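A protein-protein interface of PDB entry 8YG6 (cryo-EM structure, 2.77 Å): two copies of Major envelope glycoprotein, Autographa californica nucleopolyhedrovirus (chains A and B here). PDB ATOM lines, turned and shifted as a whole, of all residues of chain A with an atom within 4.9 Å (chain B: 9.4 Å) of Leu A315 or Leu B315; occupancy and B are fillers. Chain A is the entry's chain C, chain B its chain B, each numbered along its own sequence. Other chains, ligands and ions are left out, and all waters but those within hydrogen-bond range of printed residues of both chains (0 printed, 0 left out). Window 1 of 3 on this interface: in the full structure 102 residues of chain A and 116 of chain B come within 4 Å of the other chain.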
ATOM      1  N   MET A 311      13.622  15.317  29.000  1.00  0.00           N
ATOM      2  CA  MET A 311      14.453  14.182  28.611  1.00  0.00           C
ATOM      3  C   MET A 311      15.833  14.637  28.151  1.00  0.00           C
ATOM      4  O   MET A 311      16.848  14.021  28.502  1.00  0.00           O
ATOM      5  CB  MET A 311      13.757  13.366  27.521  1.00  0.00           C
ATOM      6  CG  MET A 311      14.066  11.879  27.583  1.00  0.00           C
ATOM      7  SD  MET A 311      12.796  10.862  26.807  1.00  0.00           S
ATOM      8  CE  MET A 311      13.297  10.937  25.092  1.00  0.00           C
ATOM      9  N   LEU A 312      15.894  15.719  27.370  1.00  0.00           N
ATOM     10  CA  LEU A 312      17.184  16.205  26.885  1.00  0.00           C
ATOM     11  C   LEU A 312      18.066  16.686  28.032  1.00  0.00           C
ATOM     12  O   LEU A 312      19.278  16.430  28.039  1.00  0.00           O
ATOM     13  CB  LEU A 312      16.977  17.321  25.860  1.00  0.00           C
ATOM     14  CG  LEU A 312      18.166  17.658  24.953  1.00  0.00           C
ATOM     15  CD1 LEU A 312      17.677  18.111  23.587  1.00  0.00           C
ATOM     16  CD2 LEU A 312      19.059  18.722  25.571  1.00  0.00           C
ATOM     17  N   HIS A 313      17.489  17.403  29.001  1.00  0.00           N
ATOM     18  CA  HIS A 313      18.291  17.844  30.140  1.00  0.00           C
ATOM     19  C   HIS A 313      18.812  16.666  30.952  1.00  0.00           C
ATOM     20  O   HIS A 313      19.975  16.667  31.379  1.00  0.00           O
ATOM     21  CB  HIS A 313      17.500  18.802  31.025  1.00  0.00           C
ATOM     22  CG  HIS A 313      17.534  20.220  30.552  1.00  0.00           C
ATOM     23  ND1 HIS A 313      18.633  21.032  30.726  1.00  0.00           N
ATOM     24  CD2 HIS A 313      16.610  20.971  29.910  1.00  0.00           C
ATOM     25  CE1 HIS A 313      18.384  22.224  30.212  1.00  0.00           C
ATOM     26  NE2 HIS A 313      17.162  22.213  29.709  1.00  0.00           N
ATOM     27  N   ASP A 314      17.975  15.649  31.177  1.00  0.00           N
ATOM     28  CA  ASP A 314      18.465  14.463  31.876  1.00  0.00           C
ATOM     29  C   ASP A 314      19.606  13.807  31.104  1.00  0.00           C
ATOM     30  O   ASP A 314      20.616  13.396  31.695  1.00  0.00           O
ATOM     31  CB  ASP A 314      17.326  13.472  32.105  1.00  0.00           C
ATOM     32  CG  ASP A 314      16.584  13.729  33.401  1.00  0.00           C
ATOM     33  OD1 ASP A 314      16.609  14.882  33.882  1.00  0.00           O
ATOM     34  OD2 ASP A 314      15.982  12.779  33.944  1.00  0.00           O
ATOM     35  N   LEU A 315      19.465  13.718  29.779  1.00  0.00           N
ATOM     36  CA  LEU A 315      20.516  13.138  28.948  1.00  0.00           C
ATOM     37  C   LEU A 315      21.832  13.890  29.108  1.00  0.00           C
ATOM     38  O   LEU A 315      22.885  13.280  29.329  1.00  0.00           O
ATOM     39  CB  LEU A 315      20.078  13.139  27.482  1.00  0.00           C
ATOM     40  CG  LEU A 315      21.138  12.778  26.441  1.00  0.00           C
ATOM     41  CD1 LEU A 315      21.609  11.347  26.618  1.00  0.00           C
ATOM     42  CD2 LEU A 315      20.607  12.999  25.034  1.00  0.00           C
ATOM     43  N   ILE A 316      21.796  15.222  28.993  1.00  0.00           N
ATOM     44  CA  ILE A 316      23.043  15.981  29.045  1.00  0.00           C
ATOM     45  C   ILE A 316      23.665  15.902  30.434  1.00  0.00           C
ATOM     46  O   ILE A 316      24.891  15.789  30.572  1.00  0.00           O
ATOM     47  CB  ILE A 316      22.829  17.439  28.588  1.00  0.00           C
ATOM     48  CG1 ILE A 316      21.955  18.221  29.570  1.00  0.00           C
ATOM     49  CG2 ILE A 316      22.228  17.482  27.194  1.00  0.00           C
ATOM     50  CD1 ILE A 316      21.945  19.711  29.316  1.00  0.00           C
ATOM     51  N   VAL A 317      22.839  15.936  31.485  1.00  0.00           N
ATOM     52  CA  VAL A 317      23.374  15.839  32.840  1.00  0.00           C
ATOM     53  C   VAL A 317      24.066  14.499  33.043  1.00  0.00           C
ATOM     54  O   VAL A 317      25.156  14.427  33.625  1.00  0.00           O
ATOM     55  CB  VAL A 317      22.263  16.071  33.880  1.00  0.00           C
ATOM     56  CG1 VAL A 317      22.744  15.682  35.269  1.00  0.00           C
ATOM     57  CG2 VAL A 317      21.823  17.526  33.864  1.00  0.00           C
ATOM     58  N   SER A 318      23.451  13.414  32.565  1.00  0.00           N
ATOM     59  CA  SER A 318      24.072  12.101  32.722  1.00  0.00           C
ATOM     60  C   SER A 318      25.356  11.983  31.910  1.00  0.00           C
ATOM     61  O   SER A 318      26.348  11.420  32.388  1.00  0.00           O
ATOM     62  CB  SER A 318      23.085  11.002  32.331  1.00  0.00           C
ATOM     63  OG  SER A 318      23.732   9.743  32.277  1.00  0.00           O
ATOM     64  N   VAL A 319      25.363  12.507  30.680  1.00  0.00           N
ATOM     65  CA  VAL A 319      26.526  12.341  29.810  1.00  0.00           C
ATOM     66  C   VAL A 319      27.697  13.233  30.214  1.00  0.00           C
ATOM     67  O   VAL A 319      28.852  12.888  29.930  1.00  0.00           O
ATOM     68  CB  VAL A 319      26.124  12.586  28.343  1.00  0.00           C
ATOM     69  CG1 VAL A 319      27.322  12.480  27.410  1.00  0.00           C
ATOM     70  CG2 VAL A 319      25.068  11.581  27.919  1.00  0.00           C
ATOM     71  N   LEU A 326      31.685  19.365  27.847  1.00  0.00           N
ATOM     72  CA  LEU A 326      30.342  19.494  27.291  1.00  0.00           C
ATOM     73  C   LEU A 326      29.633  20.730  27.833  1.00  0.00           C
ATOM     74  O   LEU A 326      28.984  21.466  27.078  1.00  0.00           O
ATOM     75  CB  LEU A 326      29.533  18.234  27.591  1.00  0.00           C
ATOM     76  CG  LEU A 326      28.078  18.233  27.124  1.00  0.00           C
ATOM     77  CD1 LEU A 326      27.999  18.505  25.634  1.00  0.00           C
ATOM     78  CD2 LEU A 326      27.414  16.910  27.466  1.00  0.00           C
ATOM     79  N   LEU A 330      28.295  23.868  25.579  1.00  0.00           N
ATOM     80  CA  LEU A 330      26.893  24.260  25.529  1.00  0.00           C
ATOM     81  C   LEU A 330      26.675  25.698  25.982  1.00  0.00           C
ATOM     82  O   LEU A 330      25.664  26.305  25.613  1.00  0.00           O
ATOM     83  CB  LEU A 330      26.050  23.313  26.384  1.00  0.00           C
ATOM     84  CG  LEU A 330      25.714  21.966  25.747  1.00  0.00           C
ATOM     85  CD1 LEU A 330      25.225  20.984  26.797  1.00  0.00           C
ATOM     86  CD2 LEU A 330      24.682  22.139  24.645  1.00  0.00           C
ATOM     87  N   ILE B  13      22.959  22.317  37.949  1.00  0.00           N
ATOM     88  CA  ILE B  13      22.305  22.596  36.675  1.00  0.00           C
ATOM     89  C   ILE B  13      20.816  22.804  36.909  1.00  0.00           C
ATOM     90  O   ILE B  13      20.167  22.003  37.593  1.00  0.00           O
ATOM     91  CB  ILE B  13      22.552  21.457  35.671  1.00  0.00           C
ATOM     92  CG1 ILE B  13      24.040  21.349  35.343  1.00  0.00           C
ATOM     93  CG2 ILE B  13      21.745  21.679  34.402  1.00  0.00           C
ATOM     94  CD1 ILE B  13      24.402  20.107  34.562  1.00  0.00           C
ATOM     95  N   ASN B  15      17.032  23.417  35.028  1.00  0.00           N
ATOM     96  CA  ASN B  15      16.345  23.124  33.778  1.00  0.00           C
ATOM     97  C   ASN B  15      15.915  24.409  33.083  1.00  0.00           C
ATOM     98  O   ASN B  15      15.614  25.411  33.739  1.00  0.00           O
ATOM     99  CB  ASN B  15      15.128  22.238  34.041  1.00  0.00           C
ATOM    100  CG  ASN B  15      15.510  20.825  34.434  1.00  0.00           C
ATOM    101  OD1 ASN B  15      15.881  20.013  33.590  1.00  0.00           O
ATOM    102  ND2 ASN B  15      15.423  20.526  35.726  1.00  0.00           N
ATOM    103  N   LYS B 307      14.822  26.690  19.655  1.00  0.00           N
ATOM    104  CA  LYS B 307      15.822  26.688  20.720  1.00  0.00           C
ATOM    105  C   LYS B 307      16.251  25.267  21.067  1.00  0.00           C
ATOM    106  O   LYS B 307      17.449  24.978  21.219  1.00  0.00           O
ATOM    107  CB  LYS B 307      15.276  27.404  21.958  1.00  0.00           C
ATOM    108  CG  LYS B 307      16.257  27.461  23.114  1.00  0.00           C
ATOM    109  CD  LYS B 307      17.424  28.381  22.804  1.00  0.00           C
ATOM    110  CE  LYS B 307      18.433  28.391  23.941  1.00  0.00           C
ATOM    111  NZ  LYS B 307      17.856  28.945  25.195  1.00  0.00           N
ATOM    112  N   LEU B 308      15.278  24.356  21.187  1.00  0.00           N
ATOM    113  CA  LEU B 308      15.617  22.969  21.493  1.00  0.00           C
ATOM    114  C   LEU B 308      16.472  22.348  20.394  1.00  0.00           C
ATOM    115  O   LEU B 308      17.411  21.593  20.677  1.00  0.00           O
ATOM    116  CB  LEU B 308      14.348  22.146  21.714  1.00  0.00           C
ATOM    117  CG  LEU B 308      13.928  21.955  23.172  1.00  0.00           C
ATOM    118  CD1 LEU B 308      13.387  23.248  23.761  1.00  0.00           C
ATOM    119  CD2 LEU B 308      12.905  20.838  23.288  1.00  0.00           C
ATOM    120  N   ASN B 309      16.156  22.647  19.131  1.00  0.00           N
ATOM    121  CA  ASN B 309      16.931  22.101  18.021  1.00  0.00           C
ATOM    122  C   ASN B 309      18.382  22.567  18.081  1.00  0.00           C
ATOM    123  O   ASN B 309      19.317  21.771  17.899  1.00  0.00           O
ATOM    124  CB  ASN B 309      16.292  22.505  16.693  1.00  0.00           C
ATOM    125  CG  ASN B 309      17.019  21.928  15.497  1.00  0.00           C
ATOM    126  OD1 ASN B 309      17.612  20.856  15.579  1.00  0.00           O
ATOM    127  ND2 ASN B 309      16.984  22.643  14.379  1.00  0.00           N
ATOM    128  N   ASN B 310      18.588  23.864  18.332  1.00  0.00           N
ATOM    129  CA  ASN B 310      19.952  24.381  18.431  1.00  0.00           C
ATOM    130  C   ASN B 310      20.710  23.718  19.575  1.00  0.00           C
ATOM    131  O   ASN B 310      21.882  23.338  19.420  1.00  0.00           O
ATOM    132  CB  ASN B 310      19.932  25.898  18.611  1.00  0.00           C
ATOM    133  CG  ASN B 310      19.846  26.640  17.294  1.00  0.00           C
ATOM    134  OD1 ASN B 310      19.953  26.040  16.225  1.00  0.00           O
ATOM    135  ND2 ASN B 310      19.654  27.951  17.364  1.00  0.00           N
ATOM    136  N   MET B 311      20.057  23.563  20.731  1.00  0.00           N
ATOM    137  CA  MET B 311      20.723  22.927  21.862  1.00  0.00           C
ATOM    138  C   MET B 311      21.105  21.487  21.542  1.00  0.00           C
ATOM    139  O   MET B 311      22.208  21.039  21.883  1.00  0.00           O
ATOM    140  CB  MET B 311      19.832  22.991  23.103  1.00  0.00           C
ATOM    141  CG  MET B 311      20.610  23.102  24.405  1.00  0.00           C
ATOM    142  SD  MET B 311      19.650  23.842  25.739  1.00  0.00           S
ATOM    143  CE  MET B 311      18.754  22.416  26.347  1.00  0.00           C
ATOM    144  N   LEU B 312      20.212  20.746  20.881  1.00  0.00           N
ATOM    145  CA  LEU B 312      20.510  19.354  20.549  1.00  0.00           C
ATOM    146  C   LEU B 312      21.678  19.251  19.575  1.00  0.00           C
ATOM    147  O   LEU B 312      22.536  18.369  19.718  1.00  0.00           O
ATOM    148  CB  LEU B 312      19.267  18.670  19.977  1.00  0.00           C
ATOM    149  CG  LEU B 312      19.266  17.137  19.962  1.00  0.00           C
ATOM    150  CD1 LEU B 312      17.854  16.609  20.153  1.00  0.00           C
ATOM    151  CD2 LEU B 312      19.865  16.586  18.678  1.00  0.00           C
ATOM    152  N   HIS B 313      21.721  20.122  18.563  1.00  0.00           N
ATOM    153  CA  HIS B 313      22.850  20.085  17.634  1.00  0.00           C
ATOM    154  C   HIS B 313      24.164  20.412  18.330  1.00  0.00           C
ATOM    155  O   HIS B 313      25.187  19.764  18.068  1.00  0.00           O
ATOM    156  CB  HIS B 313      22.614  21.022  16.453  1.00  0.00           C
ATOM    157  CG  HIS B 313      21.793  20.415  15.361  1.00  0.00           C
ATOM    158  ND1 HIS B 313      22.308  19.494  14.474  1.00  0.00           N
ATOM    159  CD2 HIS B 313      20.498  20.591  15.012  1.00  0.00           C
ATOM    160  CE1 HIS B 313      21.364  19.131  13.625  1.00  0.00           C
ATOM    161  NE2 HIS B 313      20.256  19.781  13.929  1.00  0.00           N
ATOM    162  N   ASP B 314      24.165  21.410  19.218  1.00  0.00           N
ATOM    163  CA  ASP B 314      25.385  21.696  19.969  1.00  0.00           C
ATOM    164  C   ASP B 314      25.807  20.491  20.803  1.00  0.00           C
ATOM    165  O   ASP B 314      26.997  20.145  20.859  1.00  0.00           O
ATOM    166  CB  ASP B 314      25.189  22.925  20.854  1.00  0.00           C
ATOM    167  CG  ASP B 314      25.523  24.217  20.136  1.00  0.00           C
ATOM    168  OD1 ASP B 314      25.449  24.240  18.888  1.00  0.00           O
ATOM    169  OD2 ASP B 314      25.865  25.207  20.814  1.00  0.00           O
ATOM    170  N   LEU B 315      24.838  19.830  21.442  1.00  0.00           N
ATOM    171  CA  LEU B 315      25.137  18.644  22.239  1.00  0.00           C
ATOM    172  C   LEU B 315      25.798  17.559  21.397  1.00  0.00           C
ATOM    173  O   LEU B 315      26.832  17.003  21.785  1.00  0.00           O
ATOM    174  CB  LEU B 315      23.852  18.113  22.878  1.00  0.00           C
ATOM    175  CG  LEU B 315      23.930  16.747  23.563  1.00  0.00           C
ATOM    176  CD1 LEU B 315      24.869  16.789  24.754  1.00  0.00           C
ATOM    177  CD2 LEU B 315      22.548  16.275  23.982  1.00  0.00           C
ATOM    178  N   ILE B 316      25.211  17.238  20.240  1.00  0.00           N
ATOM    179  CA  ILE B 316      25.752  16.141  19.441  1.00  0.00           C
ATOM    180  C   ILE B 316      27.129  16.501  18.892  1.00  0.00           C
ATOM    181  O   ILE B 316      28.033  15.655  18.850  1.00  0.00           O
ATOM    182  CB  ILE B 316      24.773  15.727  18.323  1.00  0.00           C
ATOM    183  CG1 ILE B 316      24.617  16.824  17.268  1.00  0.00           C
ATOM    184  CG2 ILE B 316      23.420  15.356  18.905  1.00  0.00           C
ATOM    185  CD1 ILE B 316      23.893  16.365  16.023  1.00  0.00           C
ATOM    186  N   VAL B 317      27.322  17.761  18.484  1.00  0.00           N
ATOM    187  CA  VAL B 317      28.625  18.170  17.973  1.00  0.00           C
ATOM    188  C   VAL B 317      29.687  18.039  19.055  1.00  0.00           C
ATOM    189  O   VAL B 317      30.798  17.553  18.801  1.00  0.00           O
ATOM    190  CB  VAL B 317      28.561  19.601  17.409  1.00  0.00           C
ATOM    191  CG1 VAL B 317      29.962  20.136  17.152  1.00  0.00           C
ATOM    192  CG2 VAL B 317      27.745  19.626  16.127  1.00  0.00           C
ATOM    193  N   SER B 318      29.368  18.460  20.282  1.00  0.00           N
ATOM    194  CA  SER B 318      30.342  18.350  21.363  1.00  0.00           C
ATOM    195  C   SER B 318      30.631  16.895  21.716  1.00  0.00           C
ATOM    196  O   SER B 318      31.787  16.528  21.958  1.00  0.00           O
ATOM    197  CB  SER B 318      29.854  19.114  22.591  1.00  0.00           C
ATOM    198  OG  SER B 318      30.681  18.846  23.710  1.00  0.00           O
ATOM    199  N   VAL B 319      29.598  16.048  21.750  1.00  0.00           N
ATOM    200  CA  VAL B 319      29.788  14.663  22.179  1.00  0.00           C
ATOM    201  C   VAL B 319      30.476  13.806  21.120  1.00  0.00           C
ATOM    202  O   VAL B 319      31.131  12.815  21.468  1.00  0.00           O
ATOM    203  CB  VAL B 319      28.437  14.051  22.594  1.00  0.00           C
ATOM    204  CG1 VAL B 319      28.584  12.588  22.992  1.00  0.00           C
ATOM    205  CG2 VAL B 319      27.848  14.830  23.756  1.00  0.00           C
ATOM    206  N   ALA B 320      30.394  14.180  19.840  1.00  0.00           N
ATOM    207  CA  ALA B 320      30.913  13.316  18.783  1.00  0.00           C
ATOM    208  C   ALA B 320      32.418  13.078  18.878  1.00  0.00           C
ATOM    209  O   ALA B 320      32.925  12.152  18.234  1.00  0.00           O
ATOM    210  CB  ALA B 320      30.572  13.903  17.414  1.00  0.00           C
ATOM    211  N   LYS B 321      33.147  13.888  19.650  1.00  0.00           N
ATOM    212  CA  LYS B 321      34.597  13.715  19.740  1.00  0.00           C
ATOM    213  C   LYS B 321      34.970  12.377  20.367  1.00  0.00           C
ATOM    214  O   LYS B 321      35.887  11.697  19.894  1.00  0.00           O
ATOM    215  CB  LYS B 321      35.218  14.866  20.532  1.00  0.00           C
ATOM    216  CG  LYS B 321      34.817  16.244  20.046  1.00  0.00           C
ATOM    217  CD  LYS B 321      35.828  16.782  19.044  1.00  0.00           C
ATOM    218  CE  LYS B 321      35.433  18.163  18.551  1.00  0.00           C
ATOM    219  NZ  LYS B 321      35.271  19.123  19.678  1.00  0.00           N
ATOM    220  N   VAL B 322      34.276  11.981  21.435  1.00  0.00           N
ATOM    221  CA  VAL B 322      34.632  10.751  22.135  1.00  0.00           C
ATOM    222  C   VAL B 322      34.147   9.530  21.366  1.00  0.00           C
ATOM    223  O   VAL B 322      34.907   8.584  21.128  1.00  0.00           O
ATOM    224  CB  VAL B 322      34.071  10.772  23.570  1.00  0.00           C
ATOM    225  CG1 VAL B 322      34.473   9.507  24.312  1.00  0.00           C
ATOM    226  CG2 VAL B 322      34.554  12.009  24.309  1.00  0.00           C
ATOM    227  N   LEU B 326      29.115   8.009  16.256  1.00  0.00           N
ATOM    228  CA  LEU B 326      27.843   8.693  16.464  1.00  0.00           C
ATOM    229  C   LEU B 326      27.321   9.304  15.169  1.00  0.00           C
ATOM    230  O   LEU B 326      26.127   9.203  14.860  1.00  0.00           O
ATOM    231  CB  LEU B 326      28.001   9.766  17.541  1.00  0.00           C
ATOM    232  CG  LEU B 326      26.767  10.617  17.839  1.00  0.00           C
ATOM    233  CD1 LEU B 326      25.592   9.734  18.215  1.00  0.00           C
ATOM    234  CD2 LEU B 326      27.068  11.615  18.944  1.00  0.00           C
ATOM    235  N   LEU B 330      23.788   8.339  13.352  1.00  0.00           N
ATOM    236  CA  LEU B 330      22.732   9.314  13.117  1.00  0.00           C
ATOM    237  C   LEU B 330      22.385   9.449  11.640  1.00  0.00           C
ATOM    238  O   LEU B 330      21.275   9.886  11.314  1.00  0.00           O
ATOM    239  CB  LEU B 330      23.137  10.677  13.680  1.00  0.00           C
ATOM    240  CG  LEU B 330      22.978  10.843  15.191  1.00  0.00           C
ATOM    241  CD1 LEU B 330      23.752  12.055  15.681  1.00  0.00           C
ATOM    242  CD2 LEU B 330      21.509  10.952  15.565  1.00  0.00           C
ATOM    243  N   ILE B 391      11.268   4.214  28.181  1.00  0.00           N
ATOM    244  CA  ILE B 391      11.941   4.848  29.309  1.00  0.00           C
ATOM    245  C   ILE B 391      11.010   4.953  30.512  1.00  0.00           C
ATOM    246  O   ILE B 391      11.461   4.905  31.663  1.00  0.00           O
ATOM    247  CB  ILE B 391      12.485   6.224  28.888  1.00  0.00           C
ATOM    248  CG1 ILE B 391      13.417   6.077  27.685  1.00  0.00           C
ATOM    249  CG2 ILE B 391      13.223   6.889  30.035  1.00  0.00           C
ATOM    250  CD1 ILE B 391      14.637   5.225  27.959  1.00  0.00           C
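Among the printed residues, merely in contact across the chains: Leu A312 with Met B311 (3.8 Å), Leu A312 with Leu B312 (3.8 Å), His A313 with Asn B15 (3.3 Å), His A313 with Met B311 (3.7 Å), Leu A315 with Leu B315 (3.95 Å), Ile A316 with Leu B315 (3.4 Å), Val A317 with Ile B13 (3.7 Å), Leu A326 with Leu B315 (3.7 Å), Leu A326 with Ser B318 (3.3 Å), Leu A330 with Met B311 (3.9 Å), Leu A330 with Asp B314 (3.9 Å) and Leu A330 with Leu B315 (3.95 Å).
Of the printed residues of chain B, Leu A312 touches Met B311 (3.8 Å) and Leu B312 (3.8 Å). Leu A315 touches one residue of chain B. Leu B308 touches none of the printed residues of chain A. Printed residues of chain A within 4 Å of Met B311: Leu A312, His A313 and Leu A330. Printed residues of chain A within 4 Å of Leu B312: Leu A312 (3.8 Å). Leu B315 touches just these residues of chain A: Leu A315 (3.95 Å), Ile A316 (3.4 Å), Leu A326 (3.7 Å) and Leu A330 (3.95 Å). The nearest printed residue of chain B that does not touch Leu A312 is Leu B308 (4.5 Å).
Printed residues of chain A that touch a printed residue of chain B: Leu A312, His A313, Leu A315, Ile A316, Val A317, Leu A326 and Leu A330. Along chain B the printed residues that touch a printed residue of chain A span positions 13 to 318. Among the printed residues, 12 pairs touch across the chains. Among the printed residues, no Asp or Glu carboxylate lies within 4 Å of a Lys or Arg side-chain nitrogen of the other chain.
Leu B312 touches its own counterpart, Leu A312. His A313 touches Met B311, but with the chains exchanged Met A311 does not touch His B313 (12.5 Å). Leu A326 touches Ser B318, but with the chains exchanged Ser A318 does not touch Leu B326 (13.1 Å). Leu A330 touches Leu B315, but with the chains exchanged Leu A315 does not touch Leu B330 (9.7 Å). Positions printed for both chains: 311, 312, 313, 314, 315, 316, 317, 318, 319, 326 and 330.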
